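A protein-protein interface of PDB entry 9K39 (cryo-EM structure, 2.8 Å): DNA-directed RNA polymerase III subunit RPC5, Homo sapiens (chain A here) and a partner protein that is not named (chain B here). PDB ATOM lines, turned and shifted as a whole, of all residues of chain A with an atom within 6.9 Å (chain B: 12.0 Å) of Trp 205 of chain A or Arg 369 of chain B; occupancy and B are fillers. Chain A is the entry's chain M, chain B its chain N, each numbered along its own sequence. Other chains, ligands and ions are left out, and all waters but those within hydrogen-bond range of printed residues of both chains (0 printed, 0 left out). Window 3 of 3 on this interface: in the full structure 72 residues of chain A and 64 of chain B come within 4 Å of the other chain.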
ATOM      1  N   ALA A  47      13.892 -27.708  32.171  1.00  0.00           N
ATOM      2  CA  ALA A  47      13.455 -28.781  31.280  1.00  0.00           C
ATOM      3  C   ALA A  47      14.578 -29.103  30.307  1.00  0.00           C
ATOM      4  O   ALA A  47      14.959 -28.258  29.495  1.00  0.00           O
ATOM      5  CB  ALA A  47      12.184 -28.389  30.530  1.00  0.00           C
ATOM      6  N   LYS A  48      15.112 -30.317  30.388  1.00  0.00           N
ATOM      7  CA  LYS A  48      16.074 -30.790  29.404  1.00  0.00           C
ATOM      8  C   LYS A  48      15.334 -31.419  28.229  1.00  0.00           C
ATOM      9  O   LYS A  48      14.303 -32.073  28.402  1.00  0.00           O
ATOM     10  CB  LYS A  48      17.034 -31.803  30.031  1.00  0.00           C
ATOM     11  CG  LYS A  48      17.740 -31.289  31.278  1.00  0.00           C
ATOM     12  CD  LYS A  48      18.623 -32.358  31.902  1.00  0.00           C
ATOM     13  CE  LYS A  48      19.734 -32.778  30.955  1.00  0.00           C
ATOM     14  NZ  LYS A  48      20.617 -33.815  31.560  1.00  0.00           N
ATOM     15  N   ILE A  49      15.860 -31.207  27.024  1.00  0.00           N
ATOM     16  CA  ILE A  49      15.190 -31.691  25.820  1.00  0.00           C
ATOM     17  C   ILE A  49      16.223 -31.849  24.715  1.00  0.00           C
ATOM     18  O   ILE A  49      17.282 -31.218  24.740  1.00  0.00           O
ATOM     19  CB  ILE A  49      14.041 -30.736  25.399  1.00  0.00           C
ATOM     20  CG1 ILE A  49      13.036 -31.462  24.503  1.00  0.00           C
ATOM     21  CG2 ILE A  49      14.599 -29.513  24.688  1.00  0.00           C
ATOM     22  CD1 ILE A  49      11.895 -30.585  24.033  1.00  0.00           C
ATOM     23  N   LYS A  50      15.912 -32.711  23.750  1.00  0.00           N
ATOM     24  CA  LYS A  50      16.731 -32.909  22.560  1.00  0.00           C
ATOM     25  C   LYS A  50      15.879 -32.677  21.323  1.00  0.00           C
ATOM     26  O   LYS A  50      14.740 -33.166  21.270  1.00  0.00           O
ATOM     27  CB  LYS A  50      17.327 -34.314  22.537  1.00  0.00           C
ATOM     28  CG  LYS A  50      18.268 -34.617  23.688  1.00  0.00           C
ATOM     29  CD  LYS A  50      18.793 -36.040  23.607  1.00  0.00           C
ATOM     30  CE  LYS A  50      19.782 -36.328  24.721  1.00  0.00           C
ATOM     31  NZ  LYS A  50      20.262 -37.738  24.687  1.00  0.00           N
ATOM     32  N   PRO A  51      16.364 -31.939  20.319  1.00  0.00           N
ATOM     33  CA  PRO A  51      15.562 -31.773  19.095  1.00  0.00           C
ATOM     34  C   PRO A  51      15.301 -33.086  18.374  1.00  0.00           C
ATOM     35  O   PRO A  51      14.142 -33.425  18.104  1.00  0.00           O
ATOM     36  CB  PRO A  51      16.409 -30.805  18.256  1.00  0.00           C
ATOM     37  CG  PRO A  51      17.802 -30.965  18.775  1.00  0.00           C
ATOM     38  CD  PRO A  51      17.661 -31.244  20.240  1.00  0.00           C
ATOM     39  N   LYS A  55      13.055 -36.515  23.880  1.00  0.00           N
ATOM     40  CA  LYS A  55      12.853 -37.092  25.207  1.00  0.00           C
ATOM     41  C   LYS A  55      13.094 -35.975  26.221  1.00  0.00           C
ATOM     42  O   LYS A  55      14.246 -35.662  26.537  1.00  0.00           O
ATOM     43  CB  LYS A  55      13.778 -38.278  25.444  1.00  0.00           C
ATOM     44  CG  LYS A  55      13.562 -38.978  26.774  1.00  0.00           C
ATOM     45  CD  LYS A  55      14.415 -40.231  26.882  1.00  0.00           C
ATOM     46  CE  LYS A  55      15.897 -39.897  26.852  1.00  0.00           C
ATOM     47  NZ  LYS A  55      16.295 -39.052  28.011  1.00  0.00           N
ATOM     48  N   VAL A  56      12.012 -35.387  26.720  1.00  0.00           N
ATOM     49  CA  VAL A  56      12.095 -34.241  27.620  1.00  0.00           C
ATOM     50  C   VAL A  56      12.087 -34.726  29.063  1.00  0.00           C
ATOM     51  O   VAL A  56      11.347 -35.647  29.427  1.00  0.00           O
ATOM     52  CB  VAL A  56      10.946 -33.246  27.348  1.00  0.00           C
ATOM     53  CG1 VAL A  56       9.591 -33.920  27.495  1.00  0.00           C
ATOM     54  CG2 VAL A  56      11.049 -32.036  28.268  1.00  0.00           C
ATOM     55  N   GLU A  57      12.932 -34.111  29.886  1.00  0.00           N
ATOM     56  CA  GLU A  57      13.018 -34.395  31.314  1.00  0.00           C
ATOM     57  C   GLU A  57      12.745 -33.102  32.068  1.00  0.00           C
ATOM     58  O   GLU A  57      13.532 -32.151  31.988  1.00  0.00           O
ATOM     59  CB  GLU A  57      14.388 -34.970  31.680  1.00  0.00           C
ATOM     60  CG  GLU A  57      14.539 -35.312  33.155  1.00  0.00           C
ATOM     61  CD  GLU A  57      15.890 -35.913  33.482  1.00  0.00           C
ATOM     62  OE1 GLU A  57      16.702 -36.107  32.552  1.00  0.00           O
ATOM     63  OE2 GLU A  57      16.143 -36.193  34.674  1.00  0.00           O
ATOM     64  N   HIS A 200      21.881 -42.398  22.022  1.00  0.00           N
ATOM     65  CA  HIS A 200      20.964 -41.357  22.473  1.00  0.00           C
ATOM     66  C   HIS A 200      21.686 -40.310  23.314  1.00  0.00           C
ATOM     67  O   HIS A 200      21.439 -39.107  23.169  1.00  0.00           O
ATOM     68  CB  HIS A 200      19.810 -41.972  23.264  1.00  0.00           C
ATOM     69  CG  HIS A 200      18.807 -42.691  22.417  1.00  0.00           C
ATOM     70  ND1 HIS A 200      18.109 -42.068  21.404  1.00  0.00           N
ATOM     71  CD2 HIS A 200      18.372 -43.974  22.437  1.00  0.00           C
ATOM     72  CE1 HIS A 200      17.294 -42.939  20.833  1.00  0.00           C
ATOM     73  NE2 HIS A 200      17.437 -44.103  21.440  1.00  0.00           N
ATOM     74  N   ALA A 201      22.585 -40.750  24.198  1.00  0.00           N
ATOM     75  CA  ALA A 201      23.330 -39.822  25.039  1.00  0.00           C
ATOM     76  C   ALA A 201      24.343 -39.001  24.251  1.00  0.00           C
ATOM     77  O   ALA A 201      24.789 -37.959  24.744  1.00  0.00           O
ATOM     78  CB  ALA A 201      24.037 -40.582  26.162  1.00  0.00           C
ATOM     79  N   GLU A 202      24.726 -39.448  23.052  1.00  0.00           N
ATOM     80  CA  GLU A 202      25.674 -38.683  22.245  1.00  0.00           C
ATOM     81  C   GLU A 202      25.113 -37.320  21.860  1.00  0.00           C
ATOM     82  O   GLU A 202      25.874 -36.357  21.706  1.00  0.00           O
ATOM     83  CB  GLU A 202      26.055 -39.468  20.990  1.00  0.00           C
ATOM     84  CG  GLU A 202      27.029 -40.607  21.233  1.00  0.00           C
ATOM     85  CD  GLU A 202      27.339 -41.389  19.970  1.00  0.00           C
ATOM     86  OE1 GLU A 202      26.786 -41.044  18.904  1.00  0.00           O
ATOM     87  OE2 GLU A 202      28.136 -42.348  20.044  1.00  0.00           O
ATOM     88  N   GLU A 203      23.801 -37.214  21.697  1.00  0.00           N
ATOM     89  CA  GLU A 203      23.198 -35.940  21.339  1.00  0.00           C
ATOM     90  C   GLU A 203      23.212 -35.004  22.545  1.00  0.00           C
ATOM     91  O   GLU A 203      22.781 -35.398  23.634  1.00  0.00           O
ATOM     92  CB  GLU A 203      21.769 -36.146  20.841  1.00  0.00           C
ATOM     93  CG  GLU A 203      21.077 -34.876  20.374  1.00  0.00           C
ATOM     94  CD  GLU A 203      19.763 -35.155  19.673  1.00  0.00           C
ATOM     95  OE1 GLU A 203      19.489 -36.334  19.372  1.00  0.00           O
ATOM     96  OE2 GLU A 203      19.004 -34.194  19.423  1.00  0.00           O
ATOM     97  N   PRO A 204      23.699 -33.774  22.397  1.00  0.00           N
ATOM     98  CA  PRO A 204      23.774 -32.869  23.549  1.00  0.00           C
ATOM     99  C   PRO A 204      22.397 -32.423  24.011  1.00  0.00           C
ATOM    100  O   PRO A 204      21.440 -32.363  23.235  1.00  0.00           O
ATOM    101  CB  PRO A 204      24.591 -31.686  23.016  1.00  0.00           C
ATOM    102  CG  PRO A 204      24.344 -31.701  21.544  1.00  0.00           C
ATOM    103  CD  PRO A 204      24.217 -33.153  21.166  1.00  0.00           C
ATOM    104  N   TRP A 205      22.308 -32.109  25.301  1.00  0.00           N
ATOM    105  CA  TRP A 205      21.057 -31.664  25.893  1.00  0.00           C
ATOM    106  C   TRP A 205      20.846 -30.170  25.676  1.00  0.00           C
ATOM    107  O   TRP A 205      21.796 -29.405  25.490  1.00  0.00           O
ATOM    108  CB  TRP A 205      21.028 -31.974  27.390  1.00  0.00           C
ATOM    109  CG  TRP A 205      20.867 -33.427  27.709  1.00  0.00           C
ATOM    110  CD1 TRP A 205      21.851 -34.306  28.046  1.00  0.00           C
ATOM    111  CD2 TRP A 205      19.643 -34.170  27.722  1.00  0.00           C
ATOM    112  NE1 TRP A 205      21.316 -35.553  28.269  1.00  0.00           N
ATOM    113  CE2 TRP A 205      19.961 -35.495  28.078  1.00  0.00           C
ATOM    114  CE3 TRP A 205      18.305 -33.842  27.468  1.00  0.00           C
ATOM    115  CZ2 TRP A 205      18.994 -36.493  28.183  1.00  0.00           C
ATOM    116  CZ3 TRP A 205      17.348 -34.834  27.576  1.00  0.00           C
ATOM    117  CH2 TRP A 205      17.697 -36.145  27.928  1.00  0.00           C
ATOM    118  N   VAL A 206      19.580 -29.764  25.705  1.00  0.00           N
ATOM    119  CA  VAL A 206      19.180 -28.367  25.570  1.00  0.00           C
ATOM    120  C   VAL A 206      18.314 -28.006  26.767  1.00  0.00           C
ATOM    121  O   VAL A 206      17.336 -28.707  27.064  1.00  0.00           O
ATOM    122  CB  VAL A 206      18.424 -28.115  24.253  1.00  0.00           C
ATOM    123  CG1 VAL A 206      17.996 -26.656  24.158  1.00  0.00           C
ATOM    124  CG2 VAL A 206      19.285 -28.502  23.063  1.00  0.00           C
ATOM    125  N   HIS A 207      18.670 -26.923  27.452  1.00  0.00           N
ATOM    126  CA  HIS A 207      17.944 -26.478  28.632  1.00  0.00           C
ATOM    127  C   HIS A 207      16.884 -25.453  28.255  1.00  0.00           C
ATOM    128  O   HIS A 207      17.121 -24.572  27.424  1.00  0.00           O
ATOM    129  CB  HIS A 207      18.903 -25.879  29.662  1.00  0.00           C
ATOM    130  CG  HIS A 207      19.885 -26.862  30.220  1.00  0.00           C
ATOM    131  ND1 HIS A 207      20.831 -27.495  29.442  1.00  0.00           N
ATOM    132  CD2 HIS A 207      20.070 -27.318  31.483  1.00  0.00           C
ATOM    133  CE1 HIS A 207      21.555 -28.300  30.201  1.00  0.00           C
ATOM    134  NE2 HIS A 207      21.113 -28.211  31.442  1.00  0.00           N
ATOM    135  N   LEU A 208      15.718 -25.563  28.890  1.00  0.00           N
ATOM    136  CA  LEU A 208      14.597 -24.674  28.635  1.00  0.00           C
ATOM    137  C   LEU A 208      13.971 -24.261  29.959  1.00  0.00           C
ATOM    138  O   LEU A 208      13.924 -25.052  30.909  1.00  0.00           O
ATOM    139  CB  LEU A 208      13.526 -25.342  27.759  1.00  0.00           C
ATOM    140  CG  LEU A 208      13.930 -26.067  26.474  1.00  0.00           C
ATOM    141  CD1 LEU A 208      12.701 -26.673  25.820  1.00  0.00           C
ATOM    142  CD2 LEU A 208      14.641 -25.133  25.513  1.00  0.00           C
ATOM    143  N   HIS A 209      13.497 -23.019  30.009  1.00  0.00           N
ATOM    144  CA  HIS A 209      12.744 -22.527  31.149  1.00  0.00           C
ATOM    145  C   HIS A 209      11.267 -22.875  30.990  1.00  0.00           C
ATOM    146  O   HIS A 209      10.792 -23.211  29.901  1.00  0.00           O
ATOM    147  CB  HIS A 209      12.913 -21.015  31.296  1.00  0.00           C
ATOM    148  CG  HIS A 209      14.337 -20.556  31.237  1.00  0.00           C
ATOM    149  ND1 HIS A 209      15.041 -20.465  30.055  1.00  0.00           N
ATOM    150  CD2 HIS A 209      15.190 -20.162  32.211  1.00  0.00           C
ATOM    151  CE1 HIS A 209      16.264 -20.036  30.304  1.00  0.00           C
ATOM    152  NE2 HIS A 209      16.382 -19.843  31.606  1.00  0.00           N
ATOM    153  N   VAL B 363       6.229 -25.761  22.716  1.00  0.00           N
ATOM    154  CA  VAL B 363       7.663 -25.739  22.995  1.00  0.00           C
ATOM    155  C   VAL B 363       8.326 -25.080  21.789  1.00  0.00           C
ATOM    156  O   VAL B 363       8.618 -25.723  20.779  1.00  0.00           O
ATOM    157  CB  VAL B 363       8.214 -27.138  23.270  1.00  0.00           C
ATOM    158  CG1 VAL B 363       9.704 -27.069  23.567  1.00  0.00           C
ATOM    159  CG2 VAL B 363       7.466 -27.781  24.429  1.00  0.00           C
ATOM    160  N   GLY B 364       8.571 -23.777  21.900  1.00  0.00           N
ATOM    161  CA  GLY B 364       9.165 -23.024  20.814  1.00  0.00           C
ATOM    162  C   GLY B 364      10.637 -22.729  21.012  1.00  0.00           C
ATOM    163  O   GLY B 364      11.009 -21.961  21.905  1.00  0.00           O
ATOM    164  N   LEU B 365      11.487 -23.334  20.182  1.00  0.00           N
ATOM    165  CA  LEU B 365      12.935 -23.126  20.254  1.00  0.00           C
ATOM    166  C   LEU B 365      13.299 -21.921  19.393  1.00  0.00           C
ATOM    167  O   LEU B 365      13.751 -22.036  18.251  1.00  0.00           O
ATOM    168  CB  LEU B 365      13.686 -24.377  19.815  1.00  0.00           C
ATOM    169  CG  LEU B 365      13.683 -25.598  20.742  1.00  0.00           C
ATOM    170  CD1 LEU B 365      12.381 -26.383  20.637  1.00  0.00           C
ATOM    171  CD2 LEU B 365      14.878 -26.494  20.447  1.00  0.00           C
ATOM    172  N   GLY B 366      13.091 -20.732  19.962  1.00  0.00           N
ATOM    173  CA  GLY B 366      13.418 -19.511  19.244  1.00  0.00           C
ATOM    174  C   GLY B 366      14.908 -19.350  19.008  1.00  0.00           C
ATOM    175  O   GLY B 366      15.332 -18.876  17.951  1.00  0.00           O
ATOM    176  N   ASP B 367      15.719 -19.737  19.988  1.00  0.00           N
ATOM    177  CA  ASP B 367      17.168 -19.672  19.885  1.00  0.00           C
ATOM    178  C   ASP B 367      17.748 -21.078  19.979  1.00  0.00           C
ATOM    179  O   ASP B 367      17.149 -21.974  20.579  1.00  0.00           O
ATOM    180  CB  ASP B 367      17.764 -18.779  20.982  1.00  0.00           C
ATOM    181  CG  ASP B 367      19.233 -18.475  20.754  1.00  0.00           C
ATOM    182  OD1 ASP B 367      19.756 -18.828  19.678  1.00  0.00           O
ATOM    183  OD2 ASP B 367      19.865 -17.883  21.655  1.00  0.00           O
ATOM    184  N   SER B 368      18.925 -21.260  19.377  1.00  0.00           N
ATOM    185  CA  SER B 368      19.591 -22.556  19.396  1.00  0.00           C
ATOM    186  C   SER B 368      20.104 -22.939  20.778  1.00  0.00           C
ATOM    187  O   SER B 368      20.498 -24.094  20.975  1.00  0.00           O
ATOM    188  CB  SER B 368      20.749 -22.564  18.396  1.00  0.00           C
ATOM    189  OG  SER B 368      21.408 -23.818  18.389  1.00  0.00           O
ATOM    190  N   ARG B 369      20.114 -22.009  21.731  1.00  0.00           N
ATOM    191  CA  ARG B 369      20.573 -22.280  23.085  1.00  0.00           C
ATOM    192  C   ARG B 369      19.476 -22.166  24.134  1.00  0.00           C
ATOM    193  O   ARG B 369      19.518 -22.896  25.128  1.00  0.00           O
ATOM    194  CB  ARG B 369      21.722 -21.326  23.457  1.00  0.00           C
ATOM    195  CG  ARG B 369      22.345 -21.558  24.829  1.00  0.00           C
ATOM    196  CD  ARG B 369      23.074 -22.893  24.912  1.00  0.00           C
ATOM    197  NE  ARG B 369      22.196 -23.986  25.319  1.00  0.00           N
ATOM    198  CZ  ARG B 369      22.594 -25.245  25.477  1.00  0.00           C
ATOM    199  NH1 ARG B 369      23.860 -25.574  25.259  1.00  0.00           N
ATOM    200  NH2 ARG B 369      21.725 -26.174  25.849  1.00  0.00           N
ATOM    201  N   THR B 370      18.494 -21.291  23.936  1.00  0.00           N
ATOM    202  CA  THR B 370      17.416 -21.100  24.897  1.00  0.00           C
ATOM    203  C   THR B 370      16.085 -21.099  24.160  1.00  0.00           C
ATOM    204  O   THR B 370      15.938 -20.418  23.140  1.00  0.00           O
ATOM    205  CB  THR B 370      17.588 -19.790  25.675  1.00  0.00           C
ATOM    206  OG1 THR B 370      18.853 -19.793  26.347  1.00  0.00           O
ATOM    207  CG2 THR B 370      16.477 -19.625  26.701  1.00  0.00           C
ATOM    208  N   GLY B 371      15.120 -21.863  24.681  1.00  0.00           N
ATOM    209  CA  GLY B 371      13.797 -21.920  24.103  1.00  0.00           C
ATOM    210  C   GLY B 371      12.737 -21.648  25.157  1.00  0.00           C
ATOM    211  O   GLY B 371      13.019 -21.586  26.355  1.00  0.00           O
ATOM    212  N   GLU B 372      11.505 -21.481  24.682  1.00  0.00           N
ATOM    213  CA  GLU B 372      10.368 -21.165  25.534  1.00  0.00           C
ATOM    214  C   GLU B 372       9.336 -22.277  25.445  1.00  0.00           C
ATOM    215  O   GLU B 372       9.005 -22.738  24.347  1.00  0.00           O
ATOM    216  CB  GLU B 372       9.737 -19.827  25.132  1.00  0.00           C
ATOM    217  CG  GLU B 372      10.683 -18.642  25.207  1.00  0.00           C
ATOM    218  CD  GLU B 372      10.025 -17.345  24.782  1.00  0.00           C
ATOM    219  OE1 GLU B 372       8.841 -17.379  24.387  1.00  0.00           O
ATOM    220  OE2 GLU B 372      10.691 -16.289  24.842  1.00  0.00           O
ATOM    221  N   MET B 373       8.831 -22.704  26.599  1.00  0.00           N
ATOM    222  CA  MET B 373       7.736 -23.662  26.677  1.00  0.00           C
ATOM    223  C   MET B 373       6.482 -22.920  27.123  1.00  0.00           C
ATOM    224  O   MET B 373       6.448 -22.356  28.222  1.00  0.00           O
ATOM    225  CB  MET B 373       8.061 -24.800  27.645  1.00  0.00           C
ATOM    226  CG  MET B 373       9.311 -25.584  27.287  1.00  0.00           C
ATOM    227  SD  MET B 373       9.537 -27.001  28.374  1.00  0.00           S
ATOM    228  CE  MET B 373       9.338 -26.223  29.973  1.00  0.00           C
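The backbone NH (N) of Leu 208 of chain A is in hydrogen-bond range of the backbone carbonyl oxygen (O) of Ala 47 of chain A, at 2.9 Å. The backbone carbonyl oxygen (O) of Ile 49 of chain A sits at hydrogen-bond distance from the backbone NH (N) of Val 206 of chain A (2.9 Å).
Printed residues of chain A that touch a printed residue of chain B: Ala 47, Trp 205, Val 206, His 207, Leu 208 and His 209. Hydrophobic or aromatic side chains of chain A that line the printed part of chain B: Ala 47, His 207, Leu 208 and His 209. Of the 11 printed residues of chain B, 5 touch a printed residue of chain A. Along chain B the printed residues that touch a printed residue of chain A span positions 363 to 373.
Of chain A, only Trp 205 (3.3 Å), Val 206 (3.4 Å) and His 207 (3.5 Å) come within 4 Å of Arg 369 of chain B. No residue of chain B comes within 4 Å of Lys 48 of chain A. No residue of chain B comes within 4 Å of Ile 49 of chain A. No residue of chain B comes within 4 Å of Val 56 of chain A. Glu 57 of chain A touches none of the printed residues of chain B. Val 206 of chain A touches just one residue of chain B: Arg 369 (3.4 Å). Printed residues of chain B within 4 Å of Ala 47 of chain A: Met 373. Of the printed residues of chain B, Leu 208 of chain A touches Val 363, Gly 371 and Met 373. Gly 364 of chain B touches none of the printed residues of chain A. Asp 367 of chain B touches none of the printed residues of chain A.
Among the printed residues, pairs that only touch across the chains: His 209 of chain A with Met 373 of chain B, Val 206 of chain A with Arg 369 of chain B, Leu 208 of chain A with Gly 371 of chain B, His 207 of chain A with Arg 369 of chain B, Ala 47 of chain A with Met 373 of chain B, His 209 of chain A with Thr 370 of chain B, Leu 208 of chain A with Val 363 of chain B, Leu 208 of chain A with Met 373 of chain B and His 209 of chain A with Gly 371 of chain B.
The guanidinium group of Arg 369 of chain B sits at hydrogen-bond distance from the backbone carbonyl oxygen of Trp 205 of chain A (3.3 Å).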
